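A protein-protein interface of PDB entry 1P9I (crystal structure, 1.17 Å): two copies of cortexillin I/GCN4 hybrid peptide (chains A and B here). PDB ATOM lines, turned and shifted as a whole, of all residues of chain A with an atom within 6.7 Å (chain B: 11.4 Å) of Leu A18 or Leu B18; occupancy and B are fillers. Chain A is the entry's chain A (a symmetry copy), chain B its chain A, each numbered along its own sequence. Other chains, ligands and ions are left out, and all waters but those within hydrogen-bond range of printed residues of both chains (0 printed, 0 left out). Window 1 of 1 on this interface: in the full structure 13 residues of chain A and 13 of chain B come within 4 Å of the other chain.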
ATOM      1  N   LEU A  11     -32.530 -21.943 -31.418  1.00  0.00           N
ATOM      2  CA  LEU A  11     -32.161 -21.242 -30.209  1.00  0.00           C
ATOM      3  C   LEU A  11     -33.043 -21.649 -29.038  1.00  0.00           C
ATOM      4  O   LEU A  11     -32.558 -21.810 -27.899  1.00  0.00           O
ATOM      5  CB  LEU A  11     -32.238 -19.719 -30.406  1.00  0.00           C
ATOM      6  CG  LEU A  11     -31.023 -19.176 -31.192  1.00  0.00           C
ATOM      7  CD1 LEU A  11     -31.374 -17.764 -31.585  1.00  0.00           C
ATOM      8  CD2 LEU A  11     -29.754 -19.251 -30.372  1.00  0.00           C
ATOM      9  N   ALA A  13     -34.629 -24.510 -28.710  1.00  0.00           N
ATOM     10  CA  ALA A  13     -34.279 -25.864 -28.308  1.00  0.00           C
ATOM     11  C   ALA A  13     -32.999 -25.856 -27.470  1.00  0.00           C
ATOM     12  O   ALA A  13     -32.888 -26.550 -26.478  1.00  0.00           O
ATOM     13  CB  ALA A  13     -34.102 -26.736 -29.528  1.00  0.00           C
ATOM     14  N   GLU A  14     -31.985 -25.117 -27.912  1.00  0.00           N
ATOM     15  CA  GLU A  14     -30.720 -25.025 -27.197  1.00  0.00           C
ATOM     16  C   GLU A  14     -30.946 -24.446 -25.809  1.00  0.00           C
ATOM     17  O   GLU A  14     -30.393 -24.978 -24.847  1.00  0.00           O
ATOM     18  CB  GLU A  14     -29.725 -24.159 -27.976  1.00  0.00           C
ATOM     19  CG  GLU A  14     -28.310 -24.553 -27.593  1.00  0.00           C
ATOM     20  CD  GLU A  14     -27.360 -23.910 -28.585  1.00  0.00           C
ATOM     21  OE1 GLU A  14     -27.654 -23.971 -29.798  1.00  0.00           O
ATOM     22  OE2 GLU A  14     -26.359 -23.331 -28.146  1.00  0.00           O
ATOM     23  N   ASN A  15     -31.761 -23.388 -25.748  1.00  0.00           N
ATOM     24  CA  ASN A  15     -32.002 -22.784 -24.437  1.00  0.00           C
ATOM     25  C   ASN A  15     -32.647 -23.771 -23.489  1.00  0.00           C
ATOM     26  O   ASN A  15     -32.332 -23.820 -22.299  1.00  0.00           O
ATOM     27  CB  ASN A  15     -32.885 -21.564 -24.642  1.00  0.00           C
ATOM     28  CG  ASN A  15     -33.494 -20.717 -23.568  1.00  0.00           C
ATOM     29  OD1 ASN A  15     -34.608 -20.873 -23.018  1.00  0.00           O
ATOM     30  ND2 ASN A  15     -32.759 -19.657 -23.197  1.00  0.00           N
ATOM     31  N   LYS A  16     -33.614 -24.541 -23.993  1.00  0.00           N
ATOM     32  CA  LYS A  16     -34.268 -25.518 -23.105  1.00  0.00           C
ATOM     33  C   LYS A  16     -33.267 -26.544 -22.624  1.00  0.00           C
ATOM     34  O   LYS A  16     -33.262 -26.915 -21.436  1.00  0.00           O
ATOM     35  CB  LYS A  16     -35.427 -26.162 -23.873  1.00  0.00           C
ATOM     36  CG  LYS A  16     -36.250 -27.203 -23.153  1.00  0.00           C
ATOM     37  CD  LYS A  16     -37.226 -27.817 -24.165  1.00  0.00           C
ATOM     38  N   GLN A  17     -32.419 -27.021 -23.527  1.00  0.00           N
ATOM     39  CA  GLN A  17     -31.411 -28.008 -23.161  1.00  0.00           C
ATOM     40  C   GLN A  17     -30.437 -27.473 -22.148  1.00  0.00           C
ATOM     41  O   GLN A  17     -30.052 -28.127 -21.154  1.00  0.00           O
ATOM     42  CB  GLN A  17     -30.657 -28.468 -24.421  1.00  0.00           C
ATOM     43  N   LEU A  18     -30.002 -26.240 -22.370  1.00  0.00           N
ATOM     44  CA  LEU A  18     -29.026 -25.653 -21.444  1.00  0.00           C
ATOM     45  C   LEU A  18     -29.648 -25.455 -20.083  1.00  0.00           C
ATOM     46  O   LEU A  18     -28.990 -25.644 -19.071  1.00  0.00           O
ATOM     47  CB  LEU A  18     -28.521 -24.355 -22.012  1.00  0.00           C
ATOM     48  CG  LEU A  18     -27.587 -24.490 -23.235  1.00  0.00           C
ATOM     49  CD1 LEU A  18     -27.389 -23.166 -23.931  1.00  0.00           C
ATOM     50  CD2 LEU A  18     -26.226 -25.032 -22.770  1.00  0.00           C
ATOM     51  N   LYS A  19     -30.901 -25.020 -20.008  1.00  0.00           N
ATOM     52  CA  LYS A  19     -31.557 -24.843 -18.708  1.00  0.00           C
ATOM     53  C   LYS A  19     -31.609 -26.188 -17.986  1.00  0.00           C
ATOM     54  O   LYS A  19     -31.415 -26.237 -16.778  1.00  0.00           O
ATOM     55  CB  LYS A  19     -32.936 -24.215 -18.892  1.00  0.00           C
ATOM     56  CG  LYS A  19     -32.896 -22.734 -19.161  1.00  0.00           C
ATOM     57  CD  LYS A  19     -34.253 -22.148 -19.461  1.00  0.00           C
ATOM     58  CE  LYS A  19     -34.300 -20.628 -19.391  1.00  0.00           C
ATOM     59  NZ  LYS A  19     -35.603 -20.154 -19.961  1.00  0.00           N
ATOM     60  N   ALA A  20     -31.849 -27.283 -18.712  1.00  0.00           N
ATOM     61  CA  ALA A  20     -31.944 -28.565 -18.046  1.00  0.00           C
ATOM     62  C   ALA A  20     -30.555 -29.006 -17.583  1.00  0.00           C
ATOM     63  O   ALA A  20     -30.390 -29.621 -16.516  1.00  0.00           O
ATOM     64  CB  ALA A  20     -32.569 -29.575 -18.993  1.00  0.00           C
ATOM     65  N   LYS A  21     -29.550 -28.687 -18.400  1.00  0.00           N
ATOM     66  CA  LYS A  21     -28.184 -29.029 -18.005  1.00  0.00           C
ATOM     67  C   LYS A  21     -27.765 -28.237 -16.764  1.00  0.00           C
ATOM     68  O   LYS A  21     -27.106 -28.784 -15.871  1.00  0.00           O
ATOM     69  CB  LYS A  21     -27.253 -28.755 -19.181  1.00  0.00           C
ATOM     70  CG  LYS A  21     -25.821 -29.064 -18.866  1.00  0.00           C
ATOM     71  CD  LYS A  21     -25.592 -30.538 -18.688  1.00  0.00           C
ATOM     72  CE  LYS A  21     -24.114 -30.922 -18.742  1.00  0.00           C
ATOM     73  NZ  LYS A  21     -23.972 -32.373 -19.014  1.00  0.00           N
ATOM     74  N   VAL A  22     -28.154 -26.978 -16.716  1.00  0.00           N
ATOM     75  CA  VAL A  22     -27.901 -26.210 -15.490  1.00  0.00           C
ATOM     76  C   VAL A  22     -28.576 -26.882 -14.302  1.00  0.00           C
ATOM     77  O   VAL A  22     -27.956 -26.997 -13.248  1.00  0.00           O
ATOM     78  CB  VAL A  22     -28.356 -24.752 -15.661  1.00  0.00           C
ATOM     79  CG1 VAL A  22     -28.441 -24.010 -14.345  1.00  0.00           C
ATOM     80  CG2 VAL A  22     -27.414 -24.048 -16.631  1.00  0.00           C
ATOM     81  N   GLU A  23     -29.806 -27.353 -14.436  1.00  0.00           N
ATOM     82  CA  GLU A  23     -30.532 -27.979 -13.338  1.00  0.00           C
ATOM     83  C   GLU A  23     -29.798 -29.227 -12.889  1.00  0.00           C
ATOM     84  O   GLU A  23     -29.654 -29.499 -11.698  1.00  0.00           O
ATOM     85  CB  GLU A  23     -31.957 -28.339 -13.753  1.00  0.00           C
ATOM     86  CG  GLU A  23     -32.887 -27.171 -13.890  1.00  0.00           C
ATOM     87  CD  GLU A  23     -32.884 -26.289 -12.664  1.00  0.00           C
ATOM     88  OE1 GLU A  23     -33.200 -26.864 -11.589  1.00  0.00           O
ATOM     89  OE2 GLU A  23     -32.596 -25.087 -12.792  1.00  0.00           O
ATOM     90  N   ALA B   9     -32.384 -11.694 -30.324  1.00  0.00           N
ATOM     91  CA  ALA B   9     -31.360 -11.122 -29.507  1.00  0.00           C
ATOM     92  C   ALA B   9     -31.460 -11.591 -28.070  1.00  0.00           C
ATOM     93  O   ALA B   9     -30.470 -11.894 -27.393  1.00  0.00           O
ATOM     94  CB  ALA B   9     -31.397  -9.559 -29.568  1.00  0.00           C
ATOM     95  N   SER B  10     -32.655 -11.658 -27.549  1.00  0.00           N
ATOM     96  CA  SER B  10     -32.835 -12.088 -26.177  1.00  0.00           C
ATOM     97  C   SER B  10     -32.442 -13.561 -25.994  1.00  0.00           C
ATOM     98  O   SER B  10     -31.772 -13.913 -25.059  1.00  0.00           O
ATOM     99  CB  SER B  10     -34.319 -11.941 -25.835  1.00  0.00           C
ATOM    100  OG  SER B  10     -34.582 -12.156 -24.470  1.00  0.00           O
ATOM    101  N   LEU B  11     -32.872 -14.395 -26.940  1.00  0.00           N
ATOM    102  CA  LEU B  11     -32.516 -15.796 -26.914  1.00  0.00           C
ATOM    103  C   LEU B  11     -31.012 -15.992 -27.021  1.00  0.00           C
ATOM    104  O   LEU B  11     -30.431 -16.862 -26.340  1.00  0.00           O
ATOM    105  CB  LEU B  11     -33.219 -16.567 -28.045  1.00  0.00           C
ATOM    106  CG  LEU B  11     -34.702 -16.849 -27.718  1.00  0.00           C
ATOM    107  CD1 LEU B  11     -35.336 -17.308 -29.007  1.00  0.00           C
ATOM    108  CD2 LEU B  11     -34.842 -17.867 -26.609  1.00  0.00           C
ATOM    109  N   GLU B  12     -30.364 -15.189 -27.880  1.00  0.00           N
ATOM    110  CA  GLU B  12     -28.918 -15.282 -28.017  1.00  0.00           C
ATOM    111  C   GLU B  12     -28.222 -14.895 -26.714  1.00  0.00           C
ATOM    112  O   GLU B  12     -27.256 -15.517 -26.286  1.00  0.00           O
ATOM    113  CB  GLU B  12     -28.441 -14.416 -29.177  1.00  0.00           C
ATOM    114  CG  GLU B  12     -28.834 -15.158 -30.461  1.00  0.00           C
ATOM    115  CD  GLU B  12     -28.771 -14.353 -31.696  1.00  0.00           C
ATOM    116  OE1 GLU B  12     -28.416 -13.174 -31.571  1.00  0.00           O
ATOM    117  OE2 GLU B  12     -29.031 -14.978 -32.753  1.00  0.00           O
ATOM    118  N   ALA B  13     -28.708 -13.826 -26.123  1.00  0.00           N
ATOM    119  CA  ALA B  13     -28.091 -13.408 -24.873  1.00  0.00           C
ATOM    120  C   ALA B  13     -28.257 -14.493 -23.809  1.00  0.00           C
ATOM    121  O   ALA B  13     -27.346 -14.787 -23.057  1.00  0.00           O
ATOM    122  CB  ALA B  13     -28.705 -12.112 -24.402  1.00  0.00           C
ATOM    123  N   GLU B  14     -29.458 -15.051 -23.688  1.00  0.00           N
ATOM    124  CA  GLU B  14     -29.735 -16.099 -22.715  1.00  0.00           C
ATOM    125  C   GLU B  14     -28.857 -17.310 -22.988  1.00  0.00           C
ATOM    126  O   GLU B  14     -28.293 -17.859 -22.043  1.00  0.00           O
ATOM    127  CB  GLU B  14     -31.215 -16.497 -22.762  1.00  0.00           C
ATOM    128  CG  GLU B  14     -31.618 -17.080 -21.420  1.00  0.00           C
ATOM    129  CD  GLU B  14     -33.133 -17.178 -21.390  1.00  0.00           C
ATOM    130  OE1 GLU B  14     -33.788 -16.197 -21.801  1.00  0.00           O
ATOM    131  OE2 GLU B  14     -33.643 -18.232 -20.991  1.00  0.00           O
ATOM    132  N   ASN B  15     -28.756 -17.676 -24.271  1.00  0.00           N
ATOM    133  CA  ASN B  15     -27.932 -18.843 -24.587  1.00  0.00           C
ATOM    134  C   ASN B  15     -26.493 -18.626 -24.178  1.00  0.00           C
ATOM    135  O   ASN B  15     -25.820 -19.532 -23.682  1.00  0.00           O
ATOM    136  CB  ASN B  15     -28.045 -19.101 -26.081  1.00  0.00           C
ATOM    137  CG  ASN B  15     -27.268 -20.109 -26.869  1.00  0.00           C
ATOM    138  OD1 ASN B  15     -26.164 -19.943 -27.436  1.00  0.00           O
ATOM    139  ND2 ASN B  15     -27.863 -21.307 -26.999  1.00  0.00           N
ATOM    140  N   LYS B  16     -25.972 -17.425 -24.436  1.00  0.00           N
ATOM    141  CA  LYS B  16     -24.573 -17.169 -24.051  1.00  0.00           C
ATOM    142  C   LYS B  16     -24.414 -17.265 -22.550  1.00  0.00           C
ATOM    143  O   LYS B  16     -23.433 -17.848 -22.054  1.00  0.00           O
ATOM    144  CB  LYS B  16     -24.175 -15.787 -24.583  1.00  0.00           C
ATOM    145  CG  LYS B  16     -22.769 -15.310 -24.308  1.00  0.00           C
ATOM    146  CD  LYS B  16     -22.663 -13.855 -24.782  1.00  0.00           C
ATOM    147  N   GLN B  17     -25.356 -16.695 -21.812  1.00  0.00           N
ATOM    148  CA  GLN B  17     -25.299 -16.741 -20.355  1.00  0.00           C
ATOM    149  C   GLN B  17     -25.372 -18.148 -19.829  1.00  0.00           C
ATOM    150  O   GLN B  17     -24.637 -18.576 -18.913  1.00  0.00           O
ATOM    151  CB  GLN B  17     -26.445 -15.901 -19.766  1.00  0.00           C
ATOM    152  N   LEU B  18     -26.275 -18.926 -20.408  1.00  0.00           N
ATOM    153  CA  LEU B  18     -26.430 -20.307 -19.935  1.00  0.00           C
ATOM    154  C   LEU B  18     -25.187 -21.108 -20.232  1.00  0.00           C
ATOM    155  O   LEU B  18     -24.785 -21.943 -19.436  1.00  0.00           O
ATOM    156  CB  LEU B  18     -27.646 -20.919 -20.577  1.00  0.00           C
ATOM    157  CG  LEU B  18     -29.002 -20.375 -20.075  1.00  0.00           C
ATOM    158  CD1 LEU B  18     -30.136 -20.794 -20.978  1.00  0.00           C
ATOM    159  CD2 LEU B  18     -29.258 -20.903 -18.654  1.00  0.00           C
ATOM    160  N   LYS B  19     -24.571 -20.926 -21.395  1.00  0.00           N
ATOM    161  CA  LYS B  19     -23.340 -21.658 -21.716  1.00  0.00           C
ATOM    162  C   LYS B  19     -22.265 -21.304 -20.691  1.00  0.00           C
ATOM    163  O   LYS B  19     -21.509 -22.174 -20.277  1.00  0.00           O
ATOM    164  CB  LYS B  19     -22.909 -21.369 -23.151  1.00  0.00           C
ATOM    165  CG  LYS B  19     -23.714 -22.111 -24.185  1.00  0.00           C
ATOM    166  CD  LYS B  19     -23.361 -21.726 -25.600  1.00  0.00           C
ATOM    167  CE  LYS B  19     -23.890 -22.688 -26.655  1.00  0.00           C
ATOM    168  NZ  LYS B  19     -23.714 -22.070 -28.010  1.00  0.00           N
ATOM    169  N   ALA B  20     -22.199 -20.041 -20.260  1.00  0.00           N
ATOM    170  CA  ALA B  20     -21.164 -19.670 -19.318  1.00  0.00           C
ATOM    171  C   ALA B  20     -21.477 -20.268 -17.948  1.00  0.00           C
ATOM    172  O   ALA B  20     -20.578 -20.683 -17.197  1.00  0.00           O
ATOM    173  CB  ALA B  20     -21.060 -18.156 -19.262  1.00  0.00           C
ATOM    174  N   LYS B  21     -22.771 -20.309 -17.622  1.00  0.00           N
ATOM    175  CA  LYS B  21     -23.159 -20.912 -16.349  1.00  0.00           C
ATOM    176  C   LYS B  21     -22.847 -22.411 -16.342  1.00  0.00           C
ATOM    177  O   LYS B  21     -22.387 -22.946 -15.325  1.00  0.00           O
ATOM    178  CB  LYS B  21     -24.644 -20.651 -16.116  1.00  0.00           C
ATOM    179  CG  LYS B  21     -25.140 -21.246 -14.835  1.00  0.00           C
ATOM    180  CD  LYS B  21     -24.562 -20.554 -13.634  1.00  0.00           C
ATOM    181  CE  LYS B  21     -25.314 -20.871 -12.344  1.00  0.00           C
ATOM    182  NZ  LYS B  21     -25.011 -19.852 -11.309  1.00  0.00           N
ATOM    183  N   VAL B  22     -23.087 -23.061 -17.464  1.00  0.00           N
ATOM    184  CA  VAL B  22     -22.680 -24.469 -17.562  1.00  0.00           C
ATOM    185  C   VAL B  22     -21.179 -24.596 -17.338  1.00  0.00           C
ATOM    186  O   VAL B  22     -20.756 -25.491 -16.611  1.00  0.00           O
ATOM    187  CB  VAL B  22     -23.114 -25.066 -18.910  1.00  0.00           C
ATOM    188  CG1 VAL B  22     -22.433 -26.384 -19.209  1.00  0.00           C
ATOM    189  CG2 VAL B  22     -24.631 -25.213 -18.921  1.00  0.00           C
ATOM    190  N   GLU B  23     -20.362 -23.725 -17.911  1.00  0.00           N
ATOM    191  CA  GLU B  23     -18.913 -23.799 -17.774  1.00  0.00           C
ATOM    192  C   GLU B  23     -18.529 -23.631 -16.317  1.00  0.00           C
ATOM    193  O   GLU B  23     -17.668 -24.333 -15.790  1.00  0.00           O
ATOM    194  CB  GLU B  23     -18.223 -22.727 -18.615  1.00  0.00           C
ATOM    195  CG  GLU B  23     -18.240 -22.980 -20.093  1.00  0.00           C
ATOM    196  CD  GLU B  23     -17.730 -24.357 -20.444  1.00  0.00           C
ATOM    197  OE1 GLU B  23     -16.558 -24.611 -20.058  1.00  0.00           O
ATOM    198  OE2 GLU B  23     -18.468 -25.123 -21.086  1.00  0.00           O
ATOM    199  N   GLU B  24     -19.186 -22.696 -15.641  1.00  0.00           N
ATOM    200  CA  GLU B  24     -18.922 -22.449 -14.230  1.00  0.00           C
ATOM    201  C   GLU B  24     -19.261 -23.687 -13.432  1.00  0.00           C
ATOM    202  O   GLU B  24     -18.494 -24.171 -12.593  1.00  0.00           O
ATOM    203  CB  GLU B  24     -19.740 -21.262 -13.725  1.00  0.00           C
ATOM    204  CG  GLU B  24     -19.645 -21.142 -12.207  1.00  0.00           C
ATOM    205  CD  GLU B  24     -20.460 -20.032 -11.623  1.00  0.00           C
ATOM    206  OE1 GLU B  24     -20.945 -19.185 -12.402  1.00  0.00           O
ATOM    207  OE2 GLU B  24     -20.626 -19.893 -10.383  1.00  0.00           O
ATOM    208  N   LEU B  25     -20.463 -24.239 -13.659  1.00  0.00           N
ATOM    209  CA  LEU B  25     -20.904 -25.371 -12.839  1.00  0.00           C
ATOM    210  C   LEU B  25     -20.134 -26.632 -13.121  1.00  0.00           C
ATOM    211  O   LEU B  25     -19.844 -27.392 -12.221  1.00  0.00           O
ATOM    212  CB  LEU B  25     -22.410 -25.608 -13.029  1.00  0.00           C
ATOM    213  CG  LEU B  25     -23.291 -24.469 -12.476  1.00  0.00           C
ATOM    214  CD1 LEU B  25     -24.711 -24.746 -12.926  1.00  0.00           C
ATOM    215  CD2 LEU B  25     -23.227 -24.381 -10.964  1.00  0.00           C
ATOM    216  N   LEU B  26     -19.732 -26.859 -14.363  1.00  0.00           N
ATOM    217  CA  LEU B  26     -18.801 -27.935 -14.691  1.00  0.00           C
ATOM    218  C   LEU B  26     -17.517 -27.876 -13.886  1.00  0.00           C
ATOM    219  O   LEU B  26     -17.028 -28.835 -13.306  1.00  0.00           O
ATOM    220  CB  LEU B  26     -18.396 -27.854 -16.181  1.00  0.00           C
ATOM    221  CG  LEU B  26     -19.516 -28.259 -17.125  1.00  0.00           C
ATOM    222  CD1 LEU B  26     -19.094 -27.935 -18.545  1.00  0.00           C
ATOM    223  CD2 LEU B  26     -19.864 -29.724 -17.044  1.00  0.00           C
ATOM    224  N   ALA B  27     -16.982 -26.654 -13.896  1.00  0.00           N
ATOM    225  CA  ALA B  27     -15.716 -26.451 -13.136  1.00  0.00           C
ATOM    226  C   ALA B  27     -15.943 -26.686 -11.674  1.00  0.00           C
ATOM    227  O   ALA B  27     -15.091 -27.238 -10.937  1.00  0.00           O
ATOM    228  CB  ALA B  27     -15.204 -25.053 -13.454  1.00  0.00           C
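The side-chain amide nitrogen (ND2) of Asn B15 lies within hydrogen-bond range of the side-chain carboxylate (OE2) of Glu A14 (2.8 Å). The side-chain carboxylate of Glu B14 sits at hydrogen-bond distance from the side-chain amide nitrogen of Asn A15 (2.8 Å). OE2 of Glu A14 lies within salt-bridge range of NZ of Lys B19 (2.9 Å). OE2 of Glu B14 lies within salt-bridge range of NZ of Lys A19 (2.9 Å).
The side-chain amide oxygen (OD1) of Asn A15 sits at hydrogen-bond distance from the side-chain amino group (NZ) of Lys A19 (3.3 Å). OD1 of Asn B15 sits at hydrogen-bond distance from NZ of Lys B19 (3.3 Å).
Among the printed residues, merely in contact across the chains: Leu A11 with Glu B12 (3.8 Å), Asn A15 with Leu B18 (3.6 Å), Leu A18 with Asn B15 (3.6 Å), Leu A18 with Leu B18 (3.8 Å), Leu A18 with Lys B19 (3.8 Å), Lys A19 with Leu B18 (3.8 Å), Val A22 with Val B22 (3.8 Å) and Val A22 with Leu B25 (3.96 Å).
No residue of chain B comes within 4 Å of Gln A17. Printed residues of chain B within 4 Å of Leu A18: Asn B15 (3.6 Å), Leu B18 (3.8 Å) and Lys B19 (3.8 Å). No residue of chain B comes within 4 Å of Ala A20. Of chain B, only Val B22 and Leu B25 come within 4 Å of Val A22. Of the printed residues of chain A, Glu B14 touches Asn A15 (2.8 Å) and Lys A19 (2.9 Å). Gln B17 touches none of the printed residues of chain A. Of the printed residues of chain A, Leu B18 touches Asn A15, Leu A18 and Lys A19. Printed residues of chain A within 4 Å of Leu B25: Val A22. The nearest printed residue of chain A that does not touch Asn B15 is Leu A11 (4.4 Å).
Of the 19 printed residues of chain B, 7 touch a printed residue of chain A. Hydrophobic or aromatic side chains of chain A within 4 Å of the printed part of chain B: Leu A11, Leu A18 and Val A22. Among the printed residues, 12 pairs touch across the chains. Among the printed residues, Asp or Glu carboxylates within 4 Å of a Lys or Arg side-chain nitrogen of the other chain: Glu A14 with Lys B19 (2.9 Å) and Lys A19 with Glu B14 (2.9 Å).
Glu A14 touches Asn B15, and with the chains exchanged Asn A15 touches Glu B14. Glu A14 touches Lys B19, and with the chains exchanged Lys A19 touches Glu B14. Leu A18 touches its own counterpart, Leu B18. Val A22 touches its own counterpart, Val B22. Positions printed for both chains: 11, 13, 14, 15, 16, 17, 18, 19, 20, 21, 22 and 23.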
